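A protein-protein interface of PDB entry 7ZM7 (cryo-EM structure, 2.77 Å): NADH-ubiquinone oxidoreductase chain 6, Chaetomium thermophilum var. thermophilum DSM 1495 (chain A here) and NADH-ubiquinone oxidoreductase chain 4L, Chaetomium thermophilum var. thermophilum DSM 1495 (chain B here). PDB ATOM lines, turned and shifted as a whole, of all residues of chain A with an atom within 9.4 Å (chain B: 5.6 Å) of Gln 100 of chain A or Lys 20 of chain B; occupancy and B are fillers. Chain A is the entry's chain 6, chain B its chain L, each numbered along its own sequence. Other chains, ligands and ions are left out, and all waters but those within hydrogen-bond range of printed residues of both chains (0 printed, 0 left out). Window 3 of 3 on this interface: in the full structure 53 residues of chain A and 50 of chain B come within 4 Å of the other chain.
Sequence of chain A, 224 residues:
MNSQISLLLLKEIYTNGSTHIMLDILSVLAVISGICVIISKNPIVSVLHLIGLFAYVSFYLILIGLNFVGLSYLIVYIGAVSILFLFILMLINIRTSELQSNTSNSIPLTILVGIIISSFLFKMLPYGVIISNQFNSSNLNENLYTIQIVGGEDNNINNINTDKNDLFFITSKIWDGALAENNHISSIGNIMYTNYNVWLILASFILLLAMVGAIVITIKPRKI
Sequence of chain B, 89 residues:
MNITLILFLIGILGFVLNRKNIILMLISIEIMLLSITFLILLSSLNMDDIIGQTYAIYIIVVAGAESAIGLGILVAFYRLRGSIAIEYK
NZ of Lys 20 of chain B lies within hydrogen-bond range of O of Gln 100 of chain A. ND2 of Asn 21 of chain B lies within hydrogen-bond range of O of Leu 99 of chain A (3.0 Å).
The side-chain amide oxygen (OD1) of Asn 18 of chain B sits at hydrogen-bond distance from the backbone NH (N) of Lys 20 of chain B (3.3 Å). The backbone NH (N) of Asn 21 of chain B lies within hydrogen-bond range of the side-chain amide oxygen (OD1) of Asn 18 of chain B, 2.6 Å away.
Ile 84 of chain B touches Ile 94 of chain A. Glu 98 of chain A touches Lys 20 of chain B (O to CB, 3.4 Å). Glu 98 of chain A touches Ala 85 of chain B (CB to CB, 3.99 Å). Leu 99 of chain A touches Lys 20 of chain B. Ser 101 of chain A touches Arg 19 of chain B (CB to CB, 3.5 Å). CB of Ser 101 of chain A touches CG of Lys 20 of chain B, at 3.7 Å.
Gln 100 of chain A touches just one residue of chain B: Lys 20 (2.9 Å). Of chain A, only Glu 98 (3.4 Å), Leu 99 (3.3 Å), Gln 100 (2.9 Å) and Ser 101 (3.7 Å) come within 4 Å of Lys 20 of chain B. Of chain A, only Leu 99 (3.0 Å) comes within 4 Å of Asn 21 of chain B. No residue of chain A comes within 4 Å of Ile 86 of chain B. Of the printed residues of chain B, Glu 98 of chain A touches Lys 20 (3.4 Å) and Ala 85 (3.99 Å). Printed residues of chain B within 4 Å of Ile 94 of chain A: Ile 84 (3.95 Å). Of the printed residues of chain A, Arg 19 of chain B touches Ser 101. The nearest residue of chain B that does not touch Gln 100 of chain A is Asn 21 of chain B (5.1 Å).
Of the 9 printed residues of chain B, 5 touch a printed residue of chain A. Printed residues of chain B that touch a printed residue of chain A: Arg 19, Lys 20, Asn 21, Ile 84 and Ala 85. Among the printed residues, 8 pairs touch across the chains. Among the printed residues, no Asp or Glu carboxylate lies within 4 Å of a Lys or Arg side-chain nitrogen of the other chain.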
ATOM      1  N   ILE A  38      28.812 -12.289  12.973  1.00  0.00           N
ATOM      2  CA  ILE A  38      27.442 -12.092  13.424  1.00  0.00           C
ATOM      3  C   ILE A  38      26.572 -11.381  12.401  1.00  0.00           C
ATOM      4  O   ILE A  38      25.423 -11.046  12.710  1.00  0.00           O
ATOM      5  CB  ILE A  38      27.399 -11.317  14.758  1.00  0.00           C
ATOM      6  CG1 ILE A  38      27.922  -9.900  14.575  1.00  0.00           C
ATOM      7  CG2 ILE A  38      28.169 -12.042  15.829  1.00  0.00           C
ATOM      8  CD1 ILE A  38      27.548  -8.981  15.665  1.00  0.00           C
ATOM      9  N   ILE A  39      27.077 -11.136  11.197  1.00  0.00           N
ATOM     10  CA  ILE A  39      26.271 -10.554  10.127  1.00  0.00           C
ATOM     11  C   ILE A  39      26.141 -11.472   8.926  1.00  0.00           C
ATOM     12  O   ILE A  39      25.217 -11.281   8.121  1.00  0.00           O
ATOM     13  CB  ILE A  39      26.822  -9.186   9.683  1.00  0.00           C
ATOM     14  CG1 ILE A  39      28.170  -9.376   8.991  1.00  0.00           C
ATOM     15  CG2 ILE A  39      26.914  -8.265  10.849  1.00  0.00           C
ATOM     16  CD1 ILE A  39      28.711  -8.163   8.317  1.00  0.00           C
ATOM     17  N   SER A  40      27.011 -12.463   8.789  1.00  0.00           N
ATOM     18  CA  SER A  40      26.983 -13.364   7.650  1.00  0.00           C
ATOM     19  C   SER A  40      25.686 -14.156   7.602  1.00  0.00           C
ATOM     20  O   SER A  40      25.191 -14.637   8.627  1.00  0.00           O
ATOM     21  CB  SER A  40      28.169 -14.317   7.724  1.00  0.00           C
ATOM     22  OG  SER A  40      28.315 -15.043   6.526  1.00  0.00           O
ATOM     23  N   LYS A  41      25.138 -14.302   6.396  1.00  0.00           N
ATOM     24  CA  LYS A  41      23.893 -15.039   6.215  1.00  0.00           C
ATOM     25  C   LYS A  41      24.093 -16.537   6.405  1.00  0.00           C
ATOM     26  O   LYS A  41      23.287 -17.198   7.068  1.00  0.00           O
ATOM     27  CB  LYS A  41      23.319 -14.760   4.826  1.00  0.00           C
ATOM     28  CG  LYS A  41      22.452 -13.517   4.730  1.00  0.00           C
ATOM     29  CD  LYS A  41      23.270 -12.273   4.441  1.00  0.00           C
ATOM     30  CE  LYS A  41      22.364 -11.085   4.150  1.00  0.00           C
ATOM     31  NZ  LYS A  41      23.127  -9.821   3.963  1.00  0.00           N
ATOM     32  N   ASN A  42      25.140 -17.081   5.837  1.00  0.00           N
ATOM     33  CA  ASN A  42      25.350 -18.521   5.834  1.00  0.00           C
ATOM     34  C   ASN A  42      26.122 -18.955   7.068  1.00  0.00           C
ATOM     35  O   ASN A  42      27.196 -18.410   7.341  1.00  0.00           O
ATOM     36  CB  ASN A  42      26.110 -18.949   4.597  1.00  0.00           C
ATOM     37  CG  ASN A  42      26.373 -20.422   4.568  1.00  0.00           C
ATOM     38  OD1 ASN A  42      25.620 -21.214   5.115  1.00  0.00           O
ATOM     39  ND2 ASN A  42      27.456 -20.803   3.930  1.00  0.00           N
ATOM     40  N   PRO A  43      25.623 -19.926   7.827  1.00  0.00           N
ATOM     41  CA  PRO A  43      26.382 -20.400   8.987  1.00  0.00           C
ATOM     42  C   PRO A  43      27.729 -21.012   8.646  1.00  0.00           C
ATOM     43  O   PRO A  43      28.622 -20.999   9.499  1.00  0.00           O
ATOM     44  CB  PRO A  43      25.445 -21.418   9.634  1.00  0.00           C
ATOM     45  CG  PRO A  43      24.157 -21.248   9.016  1.00  0.00           C
ATOM     46  CD  PRO A  43      24.240 -20.410   7.817  1.00  0.00           C
ATOM     47  N   ILE A  94      20.413 -26.988   5.745  1.00  0.00           N
ATOM     48  CA  ILE A  94      20.244 -25.595   6.121  1.00  0.00           C
ATOM     49  C   ILE A  94      19.688 -24.846   4.927  1.00  0.00           C
ATOM     50  O   ILE A  94      20.360 -24.716   3.897  1.00  0.00           O
ATOM     51  CB  ILE A  94      21.560 -24.963   6.592  1.00  0.00           C
ATOM     52  CG1 ILE A  94      22.085 -25.668   7.839  1.00  0.00           C
ATOM     53  CG2 ILE A  94      21.363 -23.489   6.860  1.00  0.00           C
ATOM     54  CD1 ILE A  94      23.570 -25.872   7.843  1.00  0.00           C
ATOM     55  N   ARG A  95      18.469 -24.349   5.063  1.00  0.00           N
ATOM     56  CA  ARG A  95      17.898 -23.419   4.102  1.00  0.00           C
ATOM     57  C   ARG A  95      18.272 -22.025   4.580  1.00  0.00           C
ATOM     58  O   ARG A  95      17.821 -21.586   5.642  1.00  0.00           O
ATOM     59  CB  ARG A  95      16.389 -23.608   4.030  1.00  0.00           C
ATOM     60  CG  ARG A  95      15.950 -24.937   3.454  1.00  0.00           C
ATOM     61  CD  ARG A  95      14.432 -25.003   3.409  1.00  0.00           C
ATOM     62  NE  ARG A  95      13.933 -26.291   2.951  1.00  0.00           N
ATOM     63  CZ  ARG A  95      13.709 -26.594   1.679  1.00  0.00           C
ATOM     64  NH1 ARG A  95      13.252 -27.794   1.352  1.00  0.00           N
ATOM     65  NH2 ARG A  95      13.920 -25.687   0.738  1.00  0.00           N
ATOM     66  N   THR A  96      19.111 -21.334   3.811  1.00  0.00           N
ATOM     67  CA  THR A  96      19.801 -20.161   4.334  1.00  0.00           C
ATOM     68  C   THR A  96      18.885 -18.966   4.493  1.00  0.00           C
ATOM     69  O   THR A  96      19.317 -17.942   5.028  1.00  0.00           O
ATOM     70  CB  THR A  96      20.980 -19.796   3.432  1.00  0.00           C
ATOM     71  OG1 THR A  96      21.841 -18.871   4.109  1.00  0.00           O
ATOM     72  CG2 THR A  96      20.489 -19.155   2.147  1.00  0.00           C
ATOM     73  N   SER A  97      17.651 -19.064   4.024  1.00  0.00           N
ATOM     74  CA  SER A  97      16.673 -18.003   4.178  1.00  0.00           C
ATOM     75  C   SER A  97      15.792 -18.172   5.407  1.00  0.00           C
ATOM     76  O   SER A  97      15.217 -17.188   5.880  1.00  0.00           O
ATOM     77  CB  SER A  97      15.839 -17.940   2.910  1.00  0.00           C
ATOM     78  OG  SER A  97      15.265 -19.208   2.676  1.00  0.00           O
ATOM     79  N   GLU A  98      15.675 -19.376   5.945  1.00  0.00           N
ATOM     80  CA  GLU A  98      14.959 -19.542   7.201  1.00  0.00           C
ATOM     81  C   GLU A  98      15.774 -19.093   8.411  1.00  0.00           C
ATOM     82  O   GLU A  98      15.206 -18.917   9.491  1.00  0.00           O
ATOM     83  CB  GLU A  98      14.532 -20.996   7.383  1.00  0.00           C
ATOM     84  CG  GLU A  98      13.823 -21.588   6.195  1.00  0.00           C
ATOM     85  CD  GLU A  98      13.730 -23.105   6.263  1.00  0.00           C
ATOM     86  OE1 GLU A  98      14.722 -23.757   6.636  1.00  0.00           O
ATOM     87  OE2 GLU A  98      12.659 -23.655   5.944  1.00  0.00           O
ATOM     88  N   LEU A  99      17.079 -18.901   8.265  1.00  0.00           N
ATOM     89  CA  LEU A  99      17.893 -18.385   9.350  1.00  0.00           C
ATOM     90  C   LEU A  99      18.056 -16.881   9.283  1.00  0.00           C
ATOM     91  O   LEU A  99      18.684 -16.294  10.165  1.00  0.00           O
ATOM     92  CB  LEU A  99      19.265 -19.053   9.356  1.00  0.00           C
ATOM     93  CG  LEU A  99      19.255 -20.543   9.659  1.00  0.00           C
ATOM     94  CD1 LEU A  99      20.658 -21.035   9.939  1.00  0.00           C
ATOM     95  CD2 LEU A  99      18.359 -20.849  10.819  1.00  0.00           C
ATOM     96  N   GLN A 100      17.480 -16.245   8.278  1.00  0.00           N
ATOM     97  CA  GLN A 100      17.666 -14.824   8.054  1.00  0.00           C
ATOM     98  C   GLN A 100      16.520 -14.072   8.708  1.00  0.00           C
ATOM     99  O   GLN A 100      15.350 -14.310   8.393  1.00  0.00           O
ATOM    100  CB  GLN A 100      17.740 -14.513   6.559  1.00  0.00           C
ATOM    101  CG  GLN A 100      17.999 -13.054   6.270  1.00  0.00           C
ATOM    102  CD  GLN A 100      19.191 -12.530   7.038  1.00  0.00           C
ATOM    103  OE1 GLN A 100      20.209 -13.208   7.168  1.00  0.00           O
ATOM    104  NE2 GLN A 100      19.066 -11.319   7.565  1.00  0.00           N
ATOM    105  N   SER A 101      16.860 -13.165   9.609  1.00  0.00           N
ATOM    106  CA  SER A 101      15.889 -12.334  10.294  1.00  0.00           C
ATOM    107  C   SER A 101      16.094 -10.886   9.884  1.00  0.00           C
ATOM    108  O   SER A 101      17.149 -10.502   9.373  1.00  0.00           O
ATOM    109  CB  SER A 101      16.012 -12.489  11.809  1.00  0.00           C
ATOM    110  OG  SER A 101      17.242 -11.981  12.271  1.00  0.00           O
ATOM    111  N   ASN A 102      15.067 -10.077  10.120  1.00  0.00           N
ATOM    112  CA  ASN A 102      15.126  -8.661   9.778  1.00  0.00           C
ATOM    113  C   ASN A 102      16.116  -7.989  10.712  1.00  0.00           C
ATOM    114  O   ASN A 102      15.772  -7.599  11.828  1.00  0.00           O
ATOM    115  CB  ASN A 102      13.744  -8.031   9.890  1.00  0.00           C
ATOM    116  CG  ASN A 102      12.806  -8.502   8.808  1.00  0.00           C
ATOM    117  OD1 ASN A 102      13.142  -8.471   7.626  1.00  0.00           O
ATOM    118  ND2 ASN A 102      11.618  -8.945   9.202  1.00  0.00           N
ATOM    119  N   THR A 103      17.354  -7.844  10.247  1.00  0.00           N
ATOM    120  CA  THR A 103      18.410  -7.296  11.085  1.00  0.00           C
ATOM    121  C   THR A 103      18.280  -5.793  11.260  1.00  0.00           C
ATOM    122  O   THR A 103      18.799  -5.241  12.236  1.00  0.00           O
ATOM    123  CB  THR A 103      19.772  -7.616  10.483  1.00  0.00           C
ATOM    124  OG1 THR A 103      19.765  -7.250   9.100  1.00  0.00           O
ATOM    125  CG2 THR A 103      20.072  -9.099  10.607  1.00  0.00           C
ATOM    126  N   SER A 104      17.605  -5.122  10.326  1.00  0.00           N
ATOM    127  CA  SER A 104      17.539  -3.668  10.356  1.00  0.00           C
ATOM    128  C   SER A 104      16.743  -3.165  11.547  1.00  0.00           C
ATOM    129  O   SER A 104      16.922  -2.020  11.974  1.00  0.00           O
ATOM    130  CB  SER A 104      16.937  -3.157   9.056  1.00  0.00           C
ATOM    131  OG  SER A 104      15.730  -3.839   8.764  1.00  0.00           O
ATOM    132  N   ASN A 105      15.864  -3.998  12.093  1.00  0.00           N
ATOM    133  CA  ASN A 105      15.063  -3.589  13.237  1.00  0.00           C
ATOM    134  C   ASN A 105      15.927  -3.403  14.467  1.00  0.00           C
ATOM    135  O   ASN A 105      15.681  -2.508  15.280  1.00  0.00           O
ATOM    136  CB  ASN A 105      13.989  -4.631  13.511  1.00  0.00           C
ATOM    137  CG  ASN A 105      13.052  -4.772  12.379  1.00  0.00           C
ATOM    138  OD1 ASN A 105      12.902  -3.860  11.584  1.00  0.00           O
ATOM    139  ND2 ASN A 105      12.425  -5.925  12.271  1.00  0.00           N
ATOM    140  N   ASN B  18      19.971 -11.923  16.582  1.00  0.00           N
ATOM    141  CA  ASN B  18      19.690 -13.299  16.203  1.00  0.00           C
ATOM    142  C   ASN B  18      18.259 -13.666  16.565  1.00  0.00           C
ATOM    143  O   ASN B  18      17.943 -13.870  17.739  1.00  0.00           O
ATOM    144  CB  ASN B  18      20.675 -14.255  16.853  1.00  0.00           C
ATOM    145  CG  ASN B  18      20.666 -15.601  16.199  1.00  0.00           C
ATOM    146  OD1 ASN B  18      19.993 -15.799  15.195  1.00  0.00           O
ATOM    147  ND2 ASN B  18      21.383 -16.546  16.772  1.00  0.00           N
ATOM    148  N   ARG B  19      17.413 -13.797  15.548  1.00  0.00           N
ATOM    149  CA  ARG B  19      16.068 -14.302  15.727  1.00  0.00           C
ATOM    150  C   ARG B  19      15.892 -15.721  15.222  1.00  0.00           C
ATOM    151  O   ARG B  19      14.914 -16.373  15.596  1.00  0.00           O
ATOM    152  CB  ARG B  19      15.057 -13.402  15.007  1.00  0.00           C
ATOM    153  CG  ARG B  19      15.130 -11.951  15.390  1.00  0.00           C
ATOM    154  CD  ARG B  19      14.318 -11.640  16.633  1.00  0.00           C
ATOM    155  NE  ARG B  19      15.018 -12.011  17.862  1.00  0.00           N
ATOM    156  CZ  ARG B  19      16.083 -11.381  18.346  1.00  0.00           C
ATOM    157  NH1 ARG B  19      16.635 -11.795  19.468  1.00  0.00           N
ATOM    158  NH2 ARG B  19      16.594 -10.346  17.702  1.00  0.00           N
ATOM    159  N   LYS B  20      16.803 -16.217  14.396  1.00  0.00           N
ATOM    160  CA  LYS B  20      16.612 -17.499  13.742  1.00  0.00           C
ATOM    161  C   LYS B  20      17.777 -18.462  13.874  1.00  0.00           C
ATOM    162  O   LYS B  20      17.553 -19.670  13.744  1.00  0.00           O
ATOM    163  CB  LYS B  20      16.327 -17.287  12.255  1.00  0.00           C
ATOM    164  CG  LYS B  20      15.420 -16.129  11.966  1.00  0.00           C
ATOM    165  CD  LYS B  20      13.988 -16.542  12.066  1.00  0.00           C
ATOM    166  CE  LYS B  20      13.125 -15.642  11.213  1.00  0.00           C
ATOM    167  NZ  LYS B  20      13.333 -15.933   9.770  1.00  0.00           N
ATOM    168  N   ASN B  21      18.997 -17.985  14.117  1.00  0.00           N
ATOM    169  CA  ASN B  21      20.196 -18.823  14.119  1.00  0.00           C
ATOM    170  C   ASN B  21      20.430 -19.366  15.515  1.00  0.00           C
ATOM    171  O   ASN B  21      21.014 -18.688  16.358  1.00  0.00           O
ATOM    172  CB  ASN B  21      21.427 -18.027  13.704  1.00  0.00           C
ATOM    173  CG  ASN B  21      21.620 -17.961  12.249  1.00  0.00           C
ATOM    174  OD1 ASN B  21      22.196 -18.855  11.661  1.00  0.00           O
ATOM    175  ND2 ASN B  21      21.212 -16.865  11.651  1.00  0.00           N
ATOM    176  N   ILE B  22      20.033 -20.609  15.764  1.00  0.00           N
ATOM    177  CA  ILE B  22      20.521 -21.221  16.986  1.00  0.00           C
ATOM    178  C   ILE B  22      21.982 -21.625  16.841  1.00  0.00           C
ATOM    179  O   ILE B  22      22.622 -21.972  17.833  1.00  0.00           O
ATOM    180  CB  ILE B  22      19.635 -22.410  17.401  1.00  0.00           C
ATOM    181  CG1 ILE B  22      19.655 -23.515  16.359  1.00  0.00           C
ATOM    182  CG2 ILE B  22      18.225 -21.951  17.618  1.00  0.00           C
ATOM    183  CD1 ILE B  22      18.851 -24.694  16.761  1.00  0.00           C
ATOM    184  N   ILE B  84      16.903 -26.791  12.005  1.00  0.00           N
ATOM    185  CA  ILE B  84      17.431 -26.041  13.174  1.00  0.00           C
ATOM    186  C   ILE B  84      16.712 -24.692  13.183  1.00  0.00           C
ATOM    187  O   ILE B  84      17.046 -23.847  14.030  1.00  0.00           O
ATOM    188  CB  ILE B  84      18.956 -25.867  13.031  1.00  0.00           C
ATOM    189  CG1 ILE B  84      19.328 -25.131  11.742  1.00  0.00           C
ATOM    190  CG2 ILE B  84      19.662 -27.209  13.140  1.00  0.00           C
ATOM    191  CD1 ILE B  84      20.813 -25.007  11.524  1.00  0.00           C
ATOM    192  N   ALA B  85      15.757 -24.496  12.272  1.00  0.00           N
ATOM    193  CA  ALA B  85      15.111 -23.173  12.118  1.00  0.00           C
ATOM    194  C   ALA B  85      14.125 -22.842  13.237  1.00  0.00           C
ATOM    195  O   ALA B  85      13.602 -23.781  13.855  1.00  0.00           O
ATOM    196  CB  ALA B  85      14.447 -23.101  10.769  1.00  0.00           C
ATOM    197  N   ILE B  86      13.935 -21.548  13.511  1.00  0.00           N
ATOM    198  CA  ILE B  86      12.930 -21.107  14.521  1.00  0.00           C
ATOM    199  C   ILE B  86      11.806 -20.423  13.739  1.00  0.00           C
ATOM    200  O   ILE B  86      12.070 -19.359  13.147  1.00  0.00           O
ATOM    201  CB  ILE B  86      13.560 -20.138  15.541  1.00  0.00           C
ATOM    202  CG1 ILE B  86      14.690 -20.789  16.338  1.00  0.00           C
ATOM    203  CG2 ILE B  86      12.502 -19.545  16.459  1.00  0.00           C
ATOM    204  CD1 ILE B  86      15.003 -20.075  17.627  1.00  0.00           C
ATOM    205  N   TYR B  88       8.986 -17.947  13.012  1.00  0.00           N
ATOM    206  CA  TYR B  88       8.818 -16.613  13.646  1.00  0.00           C
ATOM    207  C   TYR B  88       7.913 -15.742  12.768  1.00  0.00           C
ATOM    208  O   TYR B  88       6.968 -15.156  13.331  1.00  0.00           O
ATOM    209  CB  TYR B  88      10.188 -15.966  13.864  1.00  0.00           C
ATOM    210  CG  TYR B  88      10.229 -14.908  14.937  1.00  0.00           C
ATOM    211  CD1 TYR B  88      10.276 -15.254  16.276  1.00  0.00           C
ATOM    212  CD2 TYR B  88      10.232 -13.561  14.614  1.00  0.00           C
ATOM    213  CE1 TYR B  88      10.317 -14.290  17.269  1.00  0.00           C
ATOM    214  CE2 TYR B  88      10.274 -12.584  15.595  1.00  0.00           C
ATOM    215  CZ  TYR B  88      10.315 -12.951  16.927  1.00  0.00           C
ATOM    216  OH  TYR B  88      10.355 -11.994  17.900  1.00  0.00           O
